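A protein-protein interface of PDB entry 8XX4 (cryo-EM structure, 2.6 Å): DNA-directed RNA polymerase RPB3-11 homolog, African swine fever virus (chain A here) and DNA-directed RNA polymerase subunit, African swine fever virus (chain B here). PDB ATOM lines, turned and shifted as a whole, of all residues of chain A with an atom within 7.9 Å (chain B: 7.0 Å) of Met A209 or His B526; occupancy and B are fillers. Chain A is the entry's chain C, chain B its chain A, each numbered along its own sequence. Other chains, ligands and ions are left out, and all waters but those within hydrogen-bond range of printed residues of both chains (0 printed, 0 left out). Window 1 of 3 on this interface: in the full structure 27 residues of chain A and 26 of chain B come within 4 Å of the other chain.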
ATOM      1  N   ARG A  51     -15.072 -40.798  11.751  1.00  0.00           N
ATOM      2  CA  ARG A  51     -15.238 -40.556  10.325  1.00  0.00           C
ATOM      3  C   ARG A  51     -14.031 -39.837   9.743  1.00  0.00           C
ATOM      4  O   ARG A  51     -13.740 -39.976   8.551  1.00  0.00           O
ATOM      5  CB  ARG A  51     -16.529 -39.767  10.090  1.00  0.00           C
ATOM      6  CG  ARG A  51     -16.516 -38.788   8.942  1.00  0.00           C
ATOM      7  CD  ARG A  51     -17.784 -37.968   8.944  1.00  0.00           C
ATOM      8  NE  ARG A  51     -17.879 -37.125  10.127  1.00  0.00           N
ATOM      9  CZ  ARG A  51     -18.970 -36.475  10.501  1.00  0.00           C
ATOM     10  NH1 ARG A  51     -20.089 -36.544   9.801  1.00  0.00           N
ATOM     11  NH2 ARG A  51     -18.940 -35.739  11.606  1.00  0.00           N
ATOM     12  N   GLN A 206     -29.998 -37.387  11.550  1.00  0.00           N
ATOM     13  CA  GLN A 206     -29.247 -36.505  12.427  1.00  0.00           C
ATOM     14  C   GLN A 206     -28.511 -35.457  11.610  1.00  0.00           C
ATOM     15  O   GLN A 206     -27.932 -35.766  10.565  1.00  0.00           O
ATOM     16  CB  GLN A 206     -28.241 -37.287  13.268  1.00  0.00           C
ATOM     17  CG  GLN A 206     -28.859 -38.260  14.235  1.00  0.00           C
ATOM     18  CD  GLN A 206     -27.836 -39.189  14.840  1.00  0.00           C
ATOM     19  OE1 GLN A 206     -26.773 -38.756  15.279  1.00  0.00           O
ATOM     20  NE2 GLN A 206     -28.149 -40.476  14.866  1.00  0.00           N
ATOM     21  N   SER A 207     -28.535 -34.219  12.089  1.00  0.00           N
ATOM     22  CA  SER A 207     -27.760 -33.166  11.453  1.00  0.00           C
ATOM     23  C   SER A 207     -26.272 -33.451  11.590  1.00  0.00           C
ATOM     24  O   SER A 207     -25.801 -33.884  12.643  1.00  0.00           O
ATOM     25  CB  SER A 207     -28.096 -31.815  12.077  1.00  0.00           C
ATOM     26  OG  SER A 207     -27.057 -30.883  11.859  1.00  0.00           O
ATOM     27  N   SER A 208     -25.527 -33.211  10.511  1.00  0.00           N
ATOM     28  CA  SER A 208     -24.088 -33.438  10.542  1.00  0.00           C
ATOM     29  C   SER A 208     -23.379 -32.506  11.508  1.00  0.00           C
ATOM     30  O   SER A 208     -22.261 -32.811  11.935  1.00  0.00           O
ATOM     31  CB  SER A 208     -23.499 -33.284   9.144  1.00  0.00           C
ATOM     32  OG  SER A 208     -24.008 -32.134   8.501  1.00  0.00           O
ATOM     33  N   MET A 209     -24.000 -31.383  11.862  1.00  0.00           N
ATOM     34  CA  MET A 209     -23.430 -30.476  12.843  1.00  0.00           C
ATOM     35  C   MET A 209     -23.448 -31.050  14.252  1.00  0.00           C
ATOM     36  O   MET A 209     -22.778 -30.504  15.130  1.00  0.00           O
ATOM     37  CB  MET A 209     -24.181 -29.148  12.813  1.00  0.00           C
ATOM     38  CG  MET A 209     -24.237 -28.502  11.447  1.00  0.00           C
ATOM     39  SD  MET A 209     -23.628 -26.809  11.432  1.00  0.00           S
ATOM     40  CE  MET A 209     -21.864 -27.054  11.555  1.00  0.00           C
ATOM     41  N   THR A 210     -24.193 -32.129  14.492  1.00  0.00           N
ATOM     42  CA  THR A 210     -24.236 -32.772  15.794  1.00  0.00           C
ATOM     43  C   THR A 210     -23.872 -34.247  15.770  1.00  0.00           C
ATOM     44  O   THR A 210     -23.428 -34.767  16.798  1.00  0.00           O
ATOM     45  CB  THR A 210     -25.632 -32.636  16.424  1.00  0.00           C
ATOM     46  OG1 THR A 210     -26.571 -33.417  15.678  1.00  0.00           O
ATOM     47  CG2 THR A 210     -26.082 -31.193  16.435  1.00  0.00           C
ATOM     48  N   SER A 211     -24.039 -34.933  14.644  1.00  0.00           N
ATOM     49  CA  SER A 211     -23.826 -36.371  14.609  1.00  0.00           C
ATOM     50  C   SER A 211     -22.344 -36.708  14.691  1.00  0.00           C
ATOM     51  O   SER A 211     -21.480 -35.951  14.244  1.00  0.00           O
ATOM     52  CB  SER A 211     -24.419 -36.969  13.339  1.00  0.00           C
ATOM     53  OG  SER A 211     -23.622 -36.651  12.218  1.00  0.00           O
ATOM     54  N   ASP A 212     -22.056 -37.862  15.286  1.00  0.00           N
ATOM     55  CA  ASP A 212     -20.702 -38.400  15.388  1.00  0.00           C
ATOM     56  C   ASP A 212     -20.759 -39.868  14.994  1.00  0.00           C
ATOM     57  O   ASP A 212     -20.795 -40.756  15.856  1.00  0.00           O
ATOM     58  CB  ASP A 212     -20.140 -38.208  16.797  1.00  0.00           C
ATOM     59  CG  ASP A 212     -18.781 -38.844  16.975  1.00  0.00           C
ATOM     60  OD1 ASP A 212     -18.015 -38.896  15.992  1.00  0.00           O
ATOM     61  OD2 ASP A 212     -18.477 -39.290  18.099  1.00  0.00           O
ATOM     62  N   PRO A 213     -20.801 -40.164  13.696  1.00  0.00           N
ATOM     63  CA  PRO A 213     -20.870 -41.563  13.268  1.00  0.00           C
ATOM     64  C   PRO A 213     -19.549 -42.280  13.481  1.00  0.00           C
ATOM     65  O   PRO A 213     -18.473 -41.727  13.249  1.00  0.00           O
ATOM     66  CB  PRO A 213     -21.216 -41.459  11.782  1.00  0.00           C
ATOM     67  CG  PRO A 213     -20.688 -40.151  11.375  1.00  0.00           C
ATOM     68  CD  PRO A 213     -20.820 -39.240  12.551  1.00  0.00           C
ATOM     69  N   LYS A 294      -7.015 -32.828  14.302  1.00  0.00           N
ATOM     70  CA  LYS A 294      -8.024 -32.106  15.064  1.00  0.00           C
ATOM     71  C   LYS A 294      -8.985 -33.065  15.749  1.00  0.00           C
ATOM     72  O   LYS A 294      -9.294 -32.902  16.933  1.00  0.00           O
ATOM     73  CB  LYS A 294      -8.779 -31.144  14.155  1.00  0.00           C
ATOM     74  CG  LYS A 294      -9.774 -30.288  14.889  1.00  0.00           C
ATOM     75  CD  LYS A 294     -10.674 -29.567  13.928  1.00  0.00           C
ATOM     76  CE  LYS A 294     -11.516 -30.531  13.127  1.00  0.00           C
ATOM     77  NZ  LYS A 294     -12.839 -29.941  12.802  1.00  0.00           N
ATOM     78  N   TYR A 298      -9.150 -33.502  19.785  1.00  0.00           N
ATOM     79  CA  TYR A 298     -10.438 -33.258  20.416  1.00  0.00           C
ATOM     80  C   TYR A 298     -10.895 -34.459  21.230  1.00  0.00           C
ATOM     81  O   TYR A 298     -11.479 -34.302  22.307  1.00  0.00           O
ATOM     82  CB  TYR A 298     -11.455 -32.916  19.337  1.00  0.00           C
ATOM     83  CG  TYR A 298     -12.812 -32.542  19.847  1.00  0.00           C
ATOM     84  CD1 TYR A 298     -12.984 -31.432  20.656  1.00  0.00           C
ATOM     85  CD2 TYR A 298     -13.928 -33.281  19.500  1.00  0.00           C
ATOM     86  CE1 TYR A 298     -14.222 -31.080  21.114  1.00  0.00           C
ATOM     87  CE2 TYR A 298     -15.168 -32.936  19.953  1.00  0.00           C
ATOM     88  CZ  TYR A 298     -15.308 -31.833  20.759  1.00  0.00           C
ATOM     89  OH  TYR A 298     -16.545 -31.479  21.211  1.00  0.00           O
ATOM     90  N   LEU B 510     -27.281 -19.949   9.309  1.00  0.00           N
ATOM     91  CA  LEU B 510     -26.612 -20.130  10.587  1.00  0.00           C
ATOM     92  C   LEU B 510     -27.448 -19.584  11.732  1.00  0.00           C
ATOM     93  O   LEU B 510     -27.565 -20.225  12.781  1.00  0.00           O
ATOM     94  CB  LEU B 510     -25.243 -19.456  10.538  1.00  0.00           C
ATOM     95  CG  LEU B 510     -24.484 -19.111  11.814  1.00  0.00           C
ATOM     96  CD1 LEU B 510     -24.058 -20.354  12.546  1.00  0.00           C
ATOM     97  CD2 LEU B 510     -23.286 -18.285  11.447  1.00  0.00           C
ATOM     98  N   ASN B 520     -31.607 -25.419  15.355  1.00  0.00           N
ATOM     99  CA  ASN B 520     -30.371 -25.110  14.643  1.00  0.00           C
ATOM    100  C   ASN B 520     -29.232 -25.065  15.655  1.00  0.00           C
ATOM    101  O   ASN B 520     -28.795 -24.008  16.113  1.00  0.00           O
ATOM    102  CB  ASN B 520     -30.510 -23.798  13.887  1.00  0.00           C
ATOM    103  CG  ASN B 520     -29.407 -23.582  12.886  1.00  0.00           C
ATOM    104  OD1 ASN B 520     -28.663 -24.499  12.556  1.00  0.00           O
ATOM    105  ND2 ASN B 520     -29.305 -22.366  12.381  1.00  0.00           N
ATOM    106  N   VAL B 521     -28.740 -26.252  16.006  1.00  0.00           N
ATOM    107  CA  VAL B 521     -27.677 -26.399  16.985  1.00  0.00           C
ATOM    108  C   VAL B 521     -26.555 -27.224  16.379  1.00  0.00           C
ATOM    109  O   VAL B 521     -26.760 -28.024  15.464  1.00  0.00           O
ATOM    110  CB  VAL B 521     -28.162 -27.051  18.294  1.00  0.00           C
ATOM    111  CG1 VAL B 521     -28.870 -26.034  19.159  1.00  0.00           C
ATOM    112  CG2 VAL B 521     -29.067 -28.227  17.996  1.00  0.00           C
ATOM    113  N   MET B 522     -25.357 -27.011  16.905  1.00  0.00           N
ATOM    114  CA  MET B 522     -24.185 -27.787  16.546  1.00  0.00           C
ATOM    115  C   MET B 522     -23.441 -28.163  17.816  1.00  0.00           C
ATOM    116  O   MET B 522     -23.537 -27.473  18.833  1.00  0.00           O
ATOM    117  CB  MET B 522     -23.261 -27.012  15.597  1.00  0.00           C
ATOM    118  CG  MET B 522     -22.581 -25.805  16.221  1.00  0.00           C
ATOM    119  SD  MET B 522     -22.605 -24.337  15.178  1.00  0.00           S
ATOM    120  CE  MET B 522     -24.317 -24.292  14.675  1.00  0.00           C
ATOM    121  N   ASN B 523     -22.707 -29.267  17.759  1.00  0.00           N
ATOM    122  CA  ASN B 523     -21.920 -29.678  18.908  1.00  0.00           C
ATOM    123  C   ASN B 523     -20.671 -28.808  19.010  1.00  0.00           C
ATOM    124  O   ASN B 523     -20.441 -27.908  18.201  1.00  0.00           O
ATOM    125  CB  ASN B 523     -21.585 -31.165  18.825  1.00  0.00           C
ATOM    126  CG  ASN B 523     -20.671 -31.498  17.674  1.00  0.00           C
ATOM    127  OD1 ASN B 523     -19.480 -31.720  17.860  1.00  0.00           O
ATOM    128  ND2 ASN B 523     -21.225 -31.552  16.479  1.00  0.00           N
ATOM    129  N   LYS B 524     -19.856 -29.067  20.033  1.00  0.00           N
ATOM    130  CA  LYS B 524     -18.718 -28.195  20.308  1.00  0.00           C
ATOM    131  C   LYS B 524     -17.692 -28.245  19.184  1.00  0.00           C
ATOM    132  O   LYS B 524     -17.062 -27.231  18.868  1.00  0.00           O
ATOM    133  CB  LYS B 524     -18.078 -28.576  21.639  1.00  0.00           C
ATOM    134  CG  LYS B 524     -16.832 -27.788  21.980  1.00  0.00           C
ATOM    135  CD  LYS B 524     -15.943 -28.578  22.906  1.00  0.00           C
ATOM    136  CE  LYS B 524     -14.674 -27.832  23.220  1.00  0.00           C
ATOM    137  NZ  LYS B 524     -14.236 -28.078  24.611  1.00  0.00           N
ATOM    138  N   LEU B 525     -17.509 -29.415  18.573  1.00  0.00           N
ATOM    139  CA  LEU B 525     -16.526 -29.544  17.504  1.00  0.00           C
ATOM    140  C   LEU B 525     -16.889 -28.682  16.305  1.00  0.00           C
ATOM    141  O   LEU B 525     -16.027 -28.012  15.728  1.00  0.00           O
ATOM    142  CB  LEU B 525     -16.393 -31.007  17.092  1.00  0.00           C
ATOM    143  CG  LEU B 525     -15.294 -31.328  16.083  1.00  0.00           C
ATOM    144  CD1 LEU B 525     -13.934 -30.984  16.649  1.00  0.00           C
ATOM    145  CD2 LEU B 525     -15.353 -32.786  15.699  1.00  0.00           C
ATOM    146  N   HIS B 526     -18.165 -28.667  15.921  1.00  0.00           N
ATOM    147  CA  HIS B 526     -18.564 -27.876  14.763  1.00  0.00           C
ATOM    148  C   HIS B 526     -18.643 -26.392  15.088  1.00  0.00           C
ATOM    149  O   HIS B 526     -18.341 -25.554  14.229  1.00  0.00           O
ATOM    150  CB  HIS B 526     -19.888 -28.396  14.221  1.00  0.00           C
ATOM    151  CG  HIS B 526     -19.753 -29.681  13.471  1.00  0.00           C
ATOM    152  ND1 HIS B 526     -19.629 -30.898  14.102  1.00  0.00           N
ATOM    153  CD2 HIS B 526     -19.679 -29.936  12.146  1.00  0.00           C
ATOM    154  CE1 HIS B 526     -19.506 -31.851  13.197  1.00  0.00           C
ATOM    155  NE2 HIS B 526     -19.534 -31.293  12.002  1.00  0.00           N
ATOM    156  N   ALA B 527     -19.018 -26.044  16.317  1.00  0.00           N
ATOM    157  CA  ALA B 527     -18.933 -24.651  16.737  1.00  0.00           C
ATOM    158  C   ALA B 527     -17.498 -24.156  16.684  1.00  0.00           C
ATOM    159  O   ALA B 527     -17.241 -23.020  16.270  1.00  0.00           O
ATOM    160  CB  ALA B 527     -19.507 -24.490  18.141  1.00  0.00           C
ATOM    161  N   MET B 528     -16.546 -24.992  17.107  1.00  0.00           N
ATOM    162  CA  MET B 528     -15.136 -24.645  16.969  1.00  0.00           C
ATOM    163  C   MET B 528     -14.741 -24.517  15.504  1.00  0.00           C
ATOM    164  O   MET B 528     -14.052 -23.566  15.120  1.00  0.00           O
ATOM    165  CB  MET B 528     -14.266 -25.694  17.659  1.00  0.00           C
ATOM    166  CG  MET B 528     -13.940 -25.386  19.099  1.00  0.00           C
ATOM    167  SD  MET B 528     -12.942 -26.636  19.920  1.00  0.00           S
ATOM    168  CE  MET B 528     -13.533 -28.122  19.128  1.00  0.00           C
ATOM    169  N   GLY B 529     -15.171 -25.465  14.672  1.00  0.00           N
ATOM    170  CA  GLY B 529     -14.811 -25.455  13.268  1.00  0.00           C
ATOM    171  C   GLY B 529     -15.376 -24.288  12.498  1.00  0.00           C
ATOM    172  O   GLY B 529     -14.868 -23.964  11.422  1.00  0.00           O
ATOM    173  N   LEU B 530     -16.434 -23.664  13.011  1.00  0.00           N
ATOM    174  CA  LEU B 530     -16.922 -22.436  12.396  1.00  0.00           C
ATOM    175  C   LEU B 530     -15.883 -21.321  12.467  1.00  0.00           C
ATOM    176  O   LEU B 530     -15.872 -20.430  11.613  1.00  0.00           O
ATOM    177  CB  LEU B 530     -18.220 -21.997  13.066  1.00  0.00           C
ATOM    178  CG  LEU B 530     -19.498 -22.209  12.262  1.00  0.00           C
ATOM    179  CD1 LEU B 530     -19.555 -23.608  11.699  1.00  0.00           C
ATOM    180  CD2 LEU B 530     -20.700 -21.942  13.129  1.00  0.00           C
ATOM    181  N   PHE B 531     -14.997 -21.360  13.458  1.00  0.00           N
ATOM    182  CA  PHE B 531     -13.994 -20.326  13.660  1.00  0.00           C
ATOM    183  C   PHE B 531     -12.627 -20.703  13.109  1.00  0.00           C
ATOM    184  O   PHE B 531     -11.660 -19.973  13.337  1.00  0.00           O
ATOM    185  CB  PHE B 531     -13.868 -20.004  15.148  1.00  0.00           C
ATOM    186  CG  PHE B 531     -15.046 -19.274  15.710  1.00  0.00           C
ATOM    187  CD1 PHE B 531     -16.133 -19.965  16.200  1.00  0.00           C
ATOM    188  CD2 PHE B 531     -15.066 -17.895  15.747  1.00  0.00           C
ATOM    189  CE1 PHE B 531     -17.211 -19.295  16.715  1.00  0.00           C
ATOM    190  CE2 PHE B 531     -16.142 -17.225  16.262  1.00  0.00           C
ATOM    191  CZ  PHE B 531     -17.216 -17.924  16.747  1.00  0.00           C
ATOM    192  N   PHE B 541     -13.863 -22.443  24.160  1.00  0.00           N
ATOM    193  CA  PHE B 541     -14.888 -23.470  24.269  1.00  0.00           C
ATOM    194  C   PHE B 541     -14.619 -24.415  25.430  1.00  0.00           C
ATOM    195  O   PHE B 541     -15.179 -25.513  25.472  1.00  0.00           O
ATOM    196  CB  PHE B 541     -14.992 -24.260  22.966  1.00  0.00           C
ATOM    197  CG  PHE B 541     -15.410 -23.440  21.788  1.00  0.00           C
ATOM    198  CD1 PHE B 541     -14.481 -22.711  21.074  1.00  0.00           C
ATOM    199  CD2 PHE B 541     -16.728 -23.408  21.386  1.00  0.00           C
ATOM    200  CE1 PHE B 541     -14.858 -21.965  19.988  1.00  0.00           C
ATOM    201  CE2 PHE B 541     -17.106 -22.659  20.303  1.00  0.00           C
ATOM    202  CZ  PHE B 541     -16.168 -21.941  19.601  1.00  0.00           C
ATOM    203  N   LEU B 549     -24.744 -28.637  22.965  1.00  0.00           N
ATOM    204  CA  LEU B 549     -25.253 -28.115  21.706  1.00  0.00           C
ATOM    205  C   LEU B 549     -25.284 -26.596  21.763  1.00  0.00           C
ATOM    206  O   LEU B 549     -25.847 -26.019  22.698  1.00  0.00           O
ATOM    207  CB  LEU B 549     -26.649 -28.661  21.408  1.00  0.00           C
ATOM    208  CG  LEU B 549     -26.780 -30.178  21.300  1.00  0.00           C
ATOM    209  CD1 LEU B 549     -28.232 -30.569  21.158  1.00  0.00           C
ATOM    210  CD2 LEU B 549     -25.971 -30.703  20.135  1.00  0.00           C
ATOM    211  N   LEU B 550     -24.689 -25.957  20.764  1.00  0.00           N
ATOM    212  CA  LEU B 550     -24.630 -24.507  20.676  1.00  0.00           C
ATOM    213  C   LEU B 550     -25.500 -24.035  19.522  1.00  0.00           C
ATOM    214  O   LEU B 550     -25.426 -24.583  18.420  1.00  0.00           O
ATOM    215  CB  LEU B 550     -23.192 -24.029  20.471  1.00  0.00           C
ATOM    216  CG  LEU B 550     -22.180 -24.253  21.591  1.00  0.00           C
ATOM    217  CD1 LEU B 550     -21.393 -25.526  21.372  1.00  0.00           C
ATOM    218  CD2 LEU B 550     -21.249 -23.067  21.668  1.00  0.00           C
ATOM    219  N   VAL B 555     -22.804 -18.815  18.633  1.00  0.00           N
ATOM    220  CA  VAL B 555     -21.496 -18.637  18.011  1.00  0.00           C
ATOM    221  C   VAL B 555     -21.410 -17.282  17.319  1.00  0.00           C
ATOM    222  O   VAL B 555     -20.346 -16.646  17.312  1.00  0.00           O
ATOM    223  CB  VAL B 555     -21.182 -19.804  17.053  1.00  0.00           C
ATOM    224  CG1 VAL B 555     -21.388 -21.130  17.755  1.00  0.00           C
ATOM    225  CG2 VAL B 555     -22.024 -19.742  15.805  1.00  0.00           C
ATOM    226  N   ASN B 642     -18.368 -21.406   6.711  1.00  0.00           N
ATOM    227  CA  ASN B 642     -18.064 -22.620   7.452  1.00  0.00           C
ATOM    228  C   ASN B 642     -19.327 -23.307   7.942  1.00  0.00           C
ATOM    229  O   ASN B 642     -19.334 -24.529   8.118  1.00  0.00           O
ATOM    230  CB  ASN B 642     -17.141 -22.298   8.623  1.00  0.00           C
ATOM    231  CG  ASN B 642     -15.770 -21.865   8.174  1.00  0.00           C
ATOM    232  OD1 ASN B 642     -15.339 -22.192   7.075  1.00  0.00           O
ATOM    233  ND2 ASN B 642     -15.075 -21.122   9.020  1.00  0.00           N
ATOM    234  N   TYR B 643     -20.397 -22.551   8.182  1.00  0.00           N
ATOM    235  CA  TYR B 643     -21.667 -23.183   8.513  1.00  0.00           C
ATOM    236  C   TYR B 643     -22.241 -23.916   7.310  1.00  0.00           C
ATOM    237  O   TYR B 643     -22.672 -25.068   7.420  1.00  0.00           O
ATOM    238  CB  TYR B 643     -22.660 -22.147   9.029  1.00  0.00           C
ATOM    239  CG  TYR B 643     -23.996 -22.747   9.378  1.00  0.00           C
ATOM    240  CD1 TYR B 643     -24.202 -23.345  10.606  1.00  0.00           C
ATOM    241  CD2 TYR B 643     -25.043 -22.731   8.476  1.00  0.00           C
ATOM    242  CE1 TYR B 643     -25.412 -23.898  10.927  1.00  0.00           C
ATOM    243  CE2 TYR B 643     -26.252 -23.286   8.790  1.00  0.00           C
ATOM    244  CZ  TYR B 643     -26.430 -23.868  10.016  1.00  0.00           C
ATOM    245  OH  TYR B 643     -27.644 -24.419  10.336  1.00  0.00           O
ATOM    246  N   VAL B 644     -22.269 -23.255   6.151  1.00  0.00           N
ATOM    247  CA  VAL B 644     -22.812 -23.890   4.955  1.00  0.00           C
ATOM    248  C   VAL B 644     -21.929 -25.042   4.490  1.00  0.00           C
ATOM    249  O   VAL B 644     -22.374 -25.892   3.714  1.00  0.00           O
ATOM    250  CB  VAL B 644     -23.016 -22.843   3.845  1.00  0.00           C
ATOM    251  CG1 VAL B 644     -23.732 -23.441   2.652  1.00  0.00           C
ATOM    252  CG2 VAL B 644     -23.815 -21.686   4.376  1.00  0.00           C
ATOM    253  N   ARG B 645     -20.682 -25.099   4.960  1.00  0.00           N
ATOM    254  CA  ARG B 645     -19.841 -26.260   4.692  1.00  0.00           C
ATOM    255  C   ARG B 645     -20.463 -27.541   5.231  1.00  0.00           C
ATOM    256  O   ARG B 645     -20.166 -28.631   4.734  1.00  0.00           O
ATOM    257  CB  ARG B 645     -18.459 -26.050   5.302  1.00  0.00           C
ATOM    258  CG  ARG B 645     -17.320 -26.422   4.387  1.00  0.00           C
ATOM    259  CD  ARG B 645     -15.995 -25.998   4.981  1.00  0.00           C
ATOM    260  NE  ARG B 645     -15.769 -24.567   4.821  1.00  0.00           N
ATOM    261  CZ  ARG B 645     -15.380 -23.994   3.691  1.00  0.00           C
ATOM    262  NH1 ARG B 645     -15.142 -24.705   2.602  1.00  0.00           N
ATOM    263  NH2 ARG B 645     -15.220 -22.674   3.657  1.00  0.00           N
ATOM    264  N   ASN B 646     -21.309 -27.434   6.249  1.00  0.00           N
ATOM    265  CA  ASN B 646     -22.046 -28.564   6.797  1.00  0.00           C
ATOM    266  C   ASN B 646     -23.518 -28.541   6.443  1.00  0.00           C
ATOM    267  O   ASN B 646     -24.106 -29.592   6.205  1.00  0.00           O
ATOM    268  CB  ASN B 646     -21.907 -28.597   8.321  1.00  0.00           C
ATOM    269  CG  ASN B 646     -20.742 -29.427   8.778  1.00  0.00           C
ATOM    270  OD1 ASN B 646     -19.653 -28.908   9.013  1.00  0.00           O
ATOM    271  ND2 ASN B 646     -20.957 -30.726   8.907  1.00  0.00           N
ATOM    272  N   ALA B 647     -24.133 -27.362   6.419  1.00  0.00           N
ATOM    273  CA  ALA B 647     -25.551 -27.274   6.096  1.00  0.00           C
ATOM    274  C   ALA B 647     -25.802 -27.617   4.636  1.00  0.00           C
ATOM    275  O   ALA B 647     -26.708 -28.389   4.316  1.00  0.00           O
ATOM    276  CB  ALA B 647     -26.076 -25.877   6.420  1.00  0.00           C
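A ring nitrogen (NE2) of His B526 is in hydrogen-bond range of the backbone carbonyl oxygen of Ser A208, 3.1 Å away.
N of Asn B523 sits at hydrogen-bond distance from O of Met A209 (2.9 Å).
ND2 of Asn B646 lies within hydrogen-bond range of OG of Ser A208, 3.4 Å away.
The backbone NH (N) of Leu B525 sits at hydrogen-bond distance from the side-chain hydroxyl (OH) of Tyr A298 (3.5 Å).
O of Met A209 sits at hydrogen-bond distance from ND1 of His B526 (3.3 Å).
OD1 of Asn B523 is in hydrogen-bond range of N of Leu B525, at 3.1 Å.
O of Met B522 lies within hydrogen-bond range of N of Leu B550 (2.7 Å).
The backbone NH (N) of Met A209 lies close to the side-chain hydroxyl (OG) of Ser A207 (3.1 Å).
The backbone carbonyl oxygen of Ser A207 lies within hydrogen-bond range of the side-chain hydroxyl of Thr A210.
The side-chain amide oxygen (OD1) of Asn B520 is in hydrogen-bond range of the side-chain hydroxyl (OH) of Tyr B643, 2.4 Å away.
NZ of Lys B524 lies within hydrogen-bond range of O of Phe B541.
O of Val B521 touches CB of Met A209 (3.9 Å).
CA of Met B522 touches O of Met A209, 3.4 Å away.
Met A209 touches Tyr B643 (SD to CE1, 3.5 Å).
CB of Asn B646 touches CE of Met A209 (3.6 Å).
Thr A210 touches Val B521 (CG2 to O, 3.4 Å).
CG2 of Thr A210 touches CA of Met B522, 3.9 Å away.
Thr A210 touches Asn B523 (CA to ND2, 3.3 Å).
Leu B549 touches Thr A210.
OH of Tyr A298 touches CB of Lys B524 (3.3 Å).
CE of Met B528 touches CE1 of Tyr A298, at 3.6 Å.
Met A209 touches just these residues of chain B: Val B521 (3.9 Å), Met B522 (3.4 Å), Asn B523 (2.3 Å), His B526 (3.3 Å), Tyr B643 (3.5 Å) and Asn B646 (3.6 Å).
Printed residues of chain A within 4 Å of Val B521: Met A209 and Thr A210.
Printed residues of chain A within 4 Å of Met B522: Met A209 (3.4 Å) and Thr A210 (3.9 Å).
Of the printed residues of chain A, Lys B524 touches Tyr A298.
Printed residues of chain A within 4 Å of Leu B525: Tyr A298 (3.5 Å).
His B526 touches two residues of chain A.
Arg B645 touches none of the printed residues of chain A.
Of the printed residues of chain A, Asn B646 touches Ser A208 (3.4 Å) and Met A209 (3.6 Å).
The nearest residue of chain B that does not touch Met A209 is Leu B530 (4.2 Å).
Hydrophobic or aromatic side chains of chain A within 4 Å of the printed part of chain B: Met A209 and Tyr A298.
Along chain A the printed residues that touch a printed residue of chain B span positions 208 to 298.
Hydrophobic or aromatic side chains of chain B within 4 Å of the printed part of chain A: Met B522, Leu B525, His B526, Met B528, Leu B549 and Tyr B643.
Among the printed residues, no Asp or Glu carboxylate lies within 4 Å of a Lys or Arg side-chain nitrogen of the other chain.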
